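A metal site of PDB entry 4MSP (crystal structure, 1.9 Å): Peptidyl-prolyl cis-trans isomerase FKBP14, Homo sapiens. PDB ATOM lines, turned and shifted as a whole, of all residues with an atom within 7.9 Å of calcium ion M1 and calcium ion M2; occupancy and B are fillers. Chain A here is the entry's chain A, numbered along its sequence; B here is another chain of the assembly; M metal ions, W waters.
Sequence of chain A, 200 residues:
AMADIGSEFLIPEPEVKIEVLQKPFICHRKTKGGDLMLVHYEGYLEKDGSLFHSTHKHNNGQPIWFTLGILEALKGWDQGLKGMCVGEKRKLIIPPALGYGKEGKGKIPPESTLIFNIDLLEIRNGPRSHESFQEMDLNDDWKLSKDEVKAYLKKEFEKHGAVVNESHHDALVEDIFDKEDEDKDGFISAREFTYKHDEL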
ATOM      1  N   ARG A 128      28.124  33.245  18.993  1.00  0.00           N
ATOM      2  CA  ARG A 128      27.300  32.166  19.526  1.00  0.00           C
ATOM      3  C   ARG A 128      27.133  32.379  21.023  1.00  0.00           C
ATOM      4  O   ARG A 128      28.126  32.529  21.720  1.00  0.00           O
ATOM      5  CB  ARG A 128      27.952  30.799  19.286  1.00  0.00           C
ATOM      6  CG  ARG A 128      27.947  30.316  17.833  1.00  0.00           C
ATOM      7  CD  ARG A 128      27.306  28.946  17.732  1.00  0.00           C
ATOM      8  NE  ARG A 128      27.167  28.484  16.358  1.00  0.00           N
ATOM      9  CZ  ARG A 128      27.817  27.447  15.837  1.00  0.00           C
ATOM     10  NH1 ARG A 128      28.671  26.746  16.594  1.00  0.00           N
ATOM     11  NH2 ARG A 128      27.620  27.092  14.569  1.00  0.00           N
ATOM     12  N   LYS A 143      23.401  18.862  24.966  1.00  0.00           N
ATOM     13  CA  LYS A 143      23.685  18.662  23.544  1.00  0.00           C
ATOM     14  C   LYS A 143      22.410  18.867  22.739  1.00  0.00           C
ATOM     15  O   LYS A 143      21.296  18.723  23.249  1.00  0.00           O
ATOM     16  CB  LYS A 143      24.317  17.285  23.276  1.00  0.00           C
ATOM     17  CG  LYS A 143      23.415  16.105  23.556  1.00  0.00           C
ATOM     18  CD  LYS A 143      24.223  14.821  23.725  1.00  0.00           C
ATOM     19  CE  LYS A 143      23.327  13.666  24.116  1.00  0.00           C
ATOM     20  NZ  LYS A 143      24.097  12.452  24.529  1.00  0.00           N
ATOM     21  N   LEU A 144      22.586  19.236  21.468  1.00  0.00           N
ATOM     22  CA  LEU A 144      21.439  19.518  20.613  1.00  0.00           C
ATOM     23  C   LEU A 144      21.209  18.350  19.675  1.00  0.00           C
ATOM     24  O   LEU A 144      22.090  18.010  18.886  1.00  0.00           O
ATOM     25  CB  LEU A 144      21.722  20.767  19.784  1.00  0.00           C
ATOM     26  CG  LEU A 144      22.232  21.973  20.572  1.00  0.00           C
ATOM     27  CD1 LEU A 144      22.413  23.168  19.657  1.00  0.00           C
ATOM     28  CD2 LEU A 144      21.273  22.299  21.697  1.00  0.00           C
ATOM     29  N   PHE A 177      24.589  19.828  10.742  1.00  0.00           N
ATOM     30  CA  PHE A 177      25.284  18.790  11.497  1.00  0.00           C
ATOM     31  C   PHE A 177      26.536  18.281  10.786  1.00  0.00           C
ATOM     32  O   PHE A 177      27.464  17.792  11.433  1.00  0.00           O
ATOM     33  CB  PHE A 177      24.356  17.628  11.854  1.00  0.00           C
ATOM     34  CG  PHE A 177      23.547  17.862  13.103  1.00  0.00           C
ATOM     35  CD1 PHE A 177      23.734  17.069  14.224  1.00  0.00           C
ATOM     36  CD2 PHE A 177      22.588  18.866  13.148  1.00  0.00           C
ATOM     37  CE1 PHE A 177      22.992  17.284  15.382  1.00  0.00           C
ATOM     38  CE2 PHE A 177      21.844  19.087  14.299  1.00  0.00           C
ATOM     39  CZ  PHE A 177      22.040  18.298  15.419  1.00  0.00           C
ATOM     40  N   LYS A 179      28.825  19.932   9.550  1.00  0.00           N
ATOM     41  CA  LYS A 179      29.938  20.718  10.078  1.00  0.00           C
ATOM     42  C   LYS A 179      30.073  20.656  11.605  1.00  0.00           C
ATOM     43  O   LYS A 179      31.179  20.548  12.122  1.00  0.00           O
ATOM     44  CB  LYS A 179      29.810  22.183   9.650  1.00  0.00           C
ATOM     45  CG  LYS A 179      30.234  22.449   8.220  1.00  0.00           C
ATOM     46  CD  LYS A 179      30.240  23.946   7.930  1.00  0.00           C
ATOM     47  CE  LYS A 179      31.114  24.708   8.924  1.00  0.00           C
ATOM     48  NZ  LYS A 179      31.156  26.166   8.629  1.00  0.00           N
ATOM     49  N   GLU A 180      28.957  20.731  12.318  1.00  0.00           N
ATOM     50  CA  GLU A 180      29.001  20.947  13.755  1.00  0.00           C
ATOM     51  C   GLU A 180      29.101  19.681  14.579  1.00  0.00           C
ATOM     52  O   GLU A 180      29.655  19.708  15.682  1.00  0.00           O
ATOM     53  CB  GLU A 180      27.791  21.790  14.213  1.00  0.00           C
ATOM     54  CG  GLU A 180      27.671  23.150  13.538  1.00  0.00           C
ATOM     55  CD  GLU A 180      28.732  24.147  14.001  1.00  0.00           C
ATOM     56  OE1 GLU A 180      29.304  23.959  15.084  1.00  0.00           O
ATOM     57  OE2 GLU A 180      28.973  25.127  13.264  1.00  0.00           O
ATOM     58  N   ASP A 181      28.562  18.581  14.074  1.00  0.00           N
ATOM     59  CA  ASP A 181      28.710  17.286  14.751  1.00  0.00           C
ATOM     60  C   ASP A 181      30.012  16.625  14.313  1.00  0.00           C
ATOM     61  O   ASP A 181      30.131  16.189  13.174  1.00  0.00           O
ATOM     62  CB  ASP A 181      27.527  16.373  14.440  1.00  0.00           C
ATOM     63  CG  ASP A 181      27.556  15.093  15.237  1.00  0.00           C
ATOM     64  OD1 ASP A 181      28.328  15.014  16.218  1.00  0.00           O
ATOM     65  OD2 ASP A 181      26.800  14.156  14.901  1.00  0.00           O
ATOM     66  N   GLU A 182      30.983  16.551  15.212  1.00  0.00           N
ATOM     67  CA  GLU A 182      32.322  16.077  14.844  1.00  0.00           C
ATOM     68  C   GLU A 182      32.533  14.605  15.143  1.00  0.00           C
ATOM     69  O   GLU A 182      33.012  13.858  14.292  1.00  0.00           O
ATOM     70  CB  GLU A 182      33.395  16.904  15.539  1.00  0.00           C
ATOM     71  CG  GLU A 182      33.455  18.350  15.082  1.00  0.00           C
ATOM     72  CD  GLU A 182      34.403  19.184  15.921  1.00  0.00           C
ATOM     73  OE1 GLU A 182      35.557  18.753  16.120  1.00  0.00           O
ATOM     74  OE2 GLU A 182      33.973  20.258  16.392  1.00  0.00           O
ATOM     75  N   ASP A 183      32.205  14.179  16.357  1.00  0.00           N
ATOM     76  CA  ASP A 183      32.313  12.753  16.690  1.00  0.00           C
ATOM     77  C   ASP A 183      31.196  11.934  16.045  1.00  0.00           C
ATOM     78  O   ASP A 183      31.227  10.700  16.066  1.00  0.00           O
ATOM     79  CB  ASP A 183      32.387  12.514  18.203  1.00  0.00           C
ATOM     80  CG  ASP A 183      31.272  13.203  18.983  1.00  0.00           C
ATOM     81  OD1 ASP A 183      31.339  13.171  20.226  1.00  0.00           O
ATOM     82  OD2 ASP A 183      30.356  13.774  18.358  1.00  0.00           O
ATOM     83  N   LYS A 184      30.220  12.638  15.467  1.00  0.00           N
ATOM     84  CA  LYS A 184      29.098  12.019  14.772  1.00  0.00           C
ATOM     85  C   LYS A 184      28.266  11.117  15.689  1.00  0.00           C
ATOM     86  O   LYS A 184      27.834  10.028  15.273  1.00  0.00           O
ATOM     87  CB  LYS A 184      29.553  11.237  13.540  1.00  0.00           C
ATOM     88  CG  LYS A 184      30.414  12.033  12.567  1.00  0.00           C
ATOM     89  CD  LYS A 184      29.716  13.303  12.106  1.00  0.00           C
ATOM     90  CE  LYS A 184      30.503  13.968  10.988  1.00  0.00           C
ATOM     91  NZ  LYS A 184      30.027  15.354  10.727  1.00  0.00           N
ATOM     92  N   ASP A 185      28.028  11.565  16.921  1.00  0.00           N
ATOM     93  CA  ASP A 185      27.111  10.846  17.790  1.00  0.00           C
ATOM     94  C   ASP A 185      25.670  11.257  17.490  1.00  0.00           C
ATOM     95  O   ASP A 185      24.728  10.737  18.074  1.00  0.00           O
ATOM     96  CB  ASP A 185      27.470  10.977  19.285  1.00  0.00           C
ATOM     97  CG  ASP A 185      27.333  12.406  19.804  1.00  0.00           C
ATOM     98  OD1 ASP A 185      27.421  13.359  19.008  1.00  0.00           O
ATOM     99  OD2 ASP A 185      27.168  12.556  21.036  1.00  0.00           O
ATOM    100  N   GLY A 186      25.522  12.192  16.549  1.00  0.00           N
ATOM    101  CA  GLY A 186      24.214  12.662  16.129  1.00  0.00           C
ATOM    102  C   GLY A 186      23.774  13.904  16.886  1.00  0.00           C
ATOM    103  O   GLY A 186      22.641  14.369  16.733  1.00  0.00           O
ATOM    104  N   PHE A 187      24.674  14.443  17.691  1.00  0.00           N
ATOM    105  CA  PHE A 187      24.377  15.601  18.516  1.00  0.00           C
ATOM    106  C   PHE A 187      25.414  16.696  18.333  1.00  0.00           C
ATOM    107  O   PHE A 187      26.517  16.457  17.852  1.00  0.00           O
ATOM    108  CB  PHE A 187      24.332  15.222  19.999  1.00  0.00           C
ATOM    109  CG  PHE A 187      23.352  14.135  20.315  1.00  0.00           C
ATOM    110  CD1 PHE A 187      23.764  12.809  20.366  1.00  0.00           C
ATOM    111  CD2 PHE A 187      22.021  14.438  20.581  1.00  0.00           C
ATOM    112  CE1 PHE A 187      22.867  11.808  20.667  1.00  0.00           C
ATOM    113  CE2 PHE A 187      21.122  13.443  20.875  1.00  0.00           C
ATOM    114  CZ  PHE A 187      21.540  12.126  20.918  1.00  0.00           C
ATOM    115  N   ILE A 188      25.047  17.904  18.730  1.00  0.00           N
ATOM    116  CA  ILE A 188      25.998  18.998  18.804  1.00  0.00           C
ATOM    117  C   ILE A 188      26.178  19.339  20.279  1.00  0.00           C
ATOM    118  O   ILE A 188      25.336  20.024  20.878  1.00  0.00           O
ATOM    119  CB  ILE A 188      25.502  20.211  18.025  1.00  0.00           C
ATOM    120  CG1 ILE A 188      25.309  19.851  16.552  1.00  0.00           C
ATOM    121  CG2 ILE A 188      26.469  21.385  18.171  1.00  0.00           C
ATOM    122  CD1 ILE A 188      24.616  20.931  15.750  1.00  0.00           C
ATOM    123  N   SER A 189      27.258  18.836  20.861  1.00  0.00           N
ATOM    124  CA  SER A 189      27.576  19.089  22.270  1.00  0.00           C
ATOM    125  C   SER A 189      27.840  20.565  22.524  1.00  0.00           C
ATOM    126  O   SER A 189      28.065  21.343  21.590  1.00  0.00           O
ATOM    127  CB  SER A 189      28.823  18.304  22.658  1.00  0.00           C
ATOM    128  OG  SER A 189      29.943  18.826  21.971  1.00  0.00           O
ATOM    129  N   ALA A 190      27.818  20.957  23.792  1.00  0.00           N
ATOM    130  CA  ALA A 190      28.122  22.342  24.159  1.00  0.00           C
ATOM    131  C   ALA A 190      29.511  22.716  23.656  1.00  0.00           C
ATOM    132  O   ALA A 190      29.721  23.830  23.158  1.00  0.00           O
ATOM    133  CB  ALA A 190      28.028  22.532  25.664  1.00  0.00           C
ATOM    134  N   ARG A 191      30.437  21.787  23.776  1.00  0.00           N
ATOM    135  CA  ARG A 191      31.793  21.973  23.281  1.00  0.00           C
ATOM    136  C   ARG A 191      31.802  22.275  21.776  1.00  0.00           C
ATOM    137  O   ARG A 191      32.366  23.290  21.351  1.00  0.00           O
ATOM    138  CB  ARG A 191      32.643  20.737  23.595  1.00  0.00           C
ATOM    139  CG  ARG A 191      34.136  20.941  23.452  1.00  0.00           C
ATOM    140  CD  ARG A 191      34.898  19.935  24.289  1.00  0.00           C
ATOM    141  NE  ARG A 191      36.348  20.049  24.089  1.00  0.00           N
ATOM    142  CZ  ARG A 191      37.038  19.287  23.242  1.00  0.00           C
ATOM    143  NH1 ARG A 191      36.421  18.363  22.519  1.00  0.00           N
ATOM    144  NH2 ARG A 191      38.351  19.460  23.124  1.00  0.00           N
ATOM    145  N   GLU A 192      31.147  21.416  20.999  1.00  0.00           N
ATOM    146  CA  GLU A 192      31.049  21.613  19.554  1.00  0.00           C
ATOM    147  C   GLU A 192      30.356  22.936  19.174  1.00  0.00           C
ATOM    148  O   GLU A 192      30.712  23.562  18.178  1.00  0.00           O
ATOM    149  CB  GLU A 192      30.319  20.435  18.894  1.00  0.00           C
ATOM    150  CG  GLU A 192      31.153  19.163  18.772  1.00  0.00           C
ATOM    151  CD  GLU A 192      30.305  17.939  18.436  1.00  0.00           C
ATOM    152  OE1 GLU A 192      29.122  17.905  18.832  1.00  0.00           O
ATOM    153  OE2 GLU A 192      30.819  17.014  17.775  1.00  0.00           O
ATOM    154  N   PHE A 193      29.380  23.354  19.980  1.00  0.00           N
ATOM    155  CA  PHE A 193      28.630  24.585  19.693  1.00  0.00           C
ATOM    156  C   PHE A 193      29.465  25.856  19.897  1.00  0.00           C
ATOM    157  O   PHE A 193      29.248  26.857  19.208  1.00  0.00           O
ATOM    158  CB  PHE A 193      27.376  24.649  20.579  1.00  0.00           C
ATOM    159  CG  PHE A 193      26.470  25.810  20.278  1.00  0.00           C
ATOM    160  CD1 PHE A 193      25.499  25.710  19.293  1.00  0.00           C
ATOM    161  CD2 PHE A 193      26.548  26.988  21.011  1.00  0.00           C
ATOM    162  CE1 PHE A 193      24.634  26.768  19.028  1.00  0.00           C
ATOM    163  CE2 PHE A 193      25.703  28.053  20.745  1.00  0.00           C
ATOM    164  CZ  PHE A 193      24.736  27.939  19.747  1.00  0.00           C
ATOM    165  N   THR A 194      30.407  25.804  20.837  1.00  0.00           N
ATOM    166  CA  THR A 194      31.174  26.973  21.277  1.00  0.00           C
ATOM    167  C   THR A 194      31.747  27.828  20.147  1.00  0.00           C
ATOM    168  O   THR A 194      31.459  29.025  20.055  1.00  0.00           O
ATOM    169  CB  THR A 194      32.331  26.563  22.212  1.00  0.00           C
ATOM    170  OG1 THR A 194      31.791  25.929  23.374  1.00  0.00           O
ATOM    171  CG2 THR A 194      33.131  27.783  22.641  1.00  0.00           C
ATOM    172  N   TYR A 195      32.547  27.221  19.280  1.00  0.00           N
ATOM    173  CA  TYR A 195      33.098  27.938  18.140  1.00  0.00           C
ATOM    174  C   TYR A 195      32.400  27.543  16.847  1.00  0.00           C
ATOM    175  O   TYR A 195      32.226  26.360  16.570  1.00  0.00           O
ATOM    176  CB  TYR A 195      34.598  27.657  18.004  1.00  0.00           C
ATOM    177  CG  TYR A 195      35.422  28.102  19.200  1.00  0.00           C
ATOM    178  CD1 TYR A 195      35.702  27.225  20.233  1.00  0.00           C
ATOM    179  CD2 TYR A 195      35.908  29.402  19.286  1.00  0.00           C
ATOM    180  CE1 TYR A 195      36.463  27.630  21.326  1.00  0.00           C
ATOM    181  CE2 TYR A 195      36.665  29.812  20.358  1.00  0.00           C
ATOM    182  CZ  TYR A 195      36.929  28.921  21.385  1.00  0.00           C
ATOM    183  OH  TYR A 195      37.680  29.321  22.465  1.00  0.00           O
ATOM    184  N   LYS A 196      31.986  28.546  16.083  1.00  0.00           N
ATOM    185  CA  LYS A 196      31.640  28.284  14.704  1.00  0.00           C
ATOM    186  C   LYS A 196      32.983  27.938  14.078  1.00  0.00           C
ATOM    187  O   LYS A 196      33.836  28.818  13.922  1.00  0.00           O
ATOM    188  CB  LYS A 196      31.090  29.535  14.015  1.00  0.00           C
ATOM    189  CG  LYS A 196      30.055  30.325  14.808  1.00  0.00           C
ATOM    190  CD  LYS A 196      29.773  31.659  14.116  1.00  0.00           C
ATOM    191  CE  LYS A 196      28.958  32.609  14.986  1.00  0.00           C
ATOM    192  NZ  LYS A 196      28.886  33.995  14.408  1.00  0.00           N
ATOM    193  N   HIS A 197      33.190  26.678  13.723  1.00  0.00           N
ATOM    194  CA  HIS A 197      34.451  26.292  13.095  1.00  0.00           C
ATOM    195  C   HIS A 197      34.520  26.806  11.659  1.00  0.00           C
ATOM    196  O   HIS A 197      35.437  26.490  10.903  1.00  0.00           O
ATOM    197  CB  HIS A 197      34.697  24.790  13.197  1.00  0.00           C
ATOM    198  CG  HIS A 197      35.057  24.326  14.574  1.00  0.00           C
ATOM    199  ND1 HIS A 197      34.122  23.792  15.451  1.00  0.00           N
ATOM    200  CD2 HIS A 197      36.234  24.333  15.251  1.00  0.00           C
ATOM    201  CE1 HIS A 197      34.720  23.489  16.592  1.00  0.00           C
ATOM    202  NE2 HIS A 197      35.992  23.799  16.494  1.00  0.00           N
ATOM    203  N   ASP A 198      33.514  27.612  11.308  1.00  0.00           N
ATOM    204  CA  ASP A 198      33.486  28.400  10.086  1.00  0.00           C
ATOM    205  C   ASP A 198      34.623  29.426  10.106  1.00  0.00           C
ATOM    206  O   ASP A 198      34.842  30.107  11.108  1.00  0.00           O
ATOM    207  CB  ASP A 198      32.134  29.102   9.976  1.00  0.00           C
ATOM    208  CG  ASP A 198      31.986  29.915   8.697  1.00  0.00           C
ATOM    209  OD1 ASP A 198      32.829  29.771   7.787  1.00  0.00           O
ATOM    210  OD2 ASP A 198      31.007  30.680   8.597  1.00  0.00           O
ATOM    211  N   GLY B 161      26.540  30.580  12.139  1.00  0.00           N
ATOM    212  CA  GLY B 161      27.653  29.767  11.687  1.00  0.00           C
ATOM    213  C   GLY B 161      27.163  28.472  11.047  1.00  0.00           C
ATOM    214  O   GLY B 161      27.886  27.469  11.034  1.00  0.00           O
HETATM  215 CA    CA M   1      31.739  23.992  16.039  1.00  0.00          CA
HETATM  216 CA    CA M   2      28.630  15.350  18.471  1.00  0.00          CA
HETATM  217  O   HOH W   1      28.264  15.033  21.025  1.00  0.00           O
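Within 4 Å of calcium ion M2: Asp 181, Asp 183, Asp 185, Phe 187 and Glu 192.
Four residues have an atom within 4 Å of calcium ion M1: Glu 180, Glu 192, Tyr 195 and His 197.
The nearest printed residue that does not touch calcium ion M1 is Arg 128 (4.2 Å).
The side-chain carboxylate (OE2) of Glu 180 is in salt-bridge range of the guanidinium group (NH2) of Arg 128 (2.7 Å).
The side-chain amino group (NZ) of Lys 184 sits at hydrogen-bond distance from the backbone carbonyl oxygen (O) of Asp 181 (2.6 Å).
OD2 of Asp 181 lies within hydrogen-bond range of N of Gly 186 (2.9 Å).
The side-chain carboxylate (OE2) of Glu 192 lies close to the backbone NH (N) of Glu 182, at 2.6 Å.
The side-chain hydroxyl of Ser 189 is in hydrogen-bond range of the backbone NH of Glu 192 (3.0 Å).
Calcium ion M2 is bound by the side-chain carboxylate (OD1) of Asp 181, the side-chain carboxylate (OD2) of Asp 183, the side-chain carboxylate (OD1) of Asp 185, the backbone carbonyl oxygen (O) of Phe 187, water W1, the side-chain carboxylate (OE1) of Glu 192 and the side-chain carboxylate (OE2) of Glu 192.
Calcium ion M1 is bound by O of Glu 192 (2.4 Å), ND1 of His 197 (2.5 Å), O of Tyr 195 (2.5 Å) and OE1 of Glu 180 (2.6 Å).
Calcium ion M1 has four donor atoms within binding distance.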
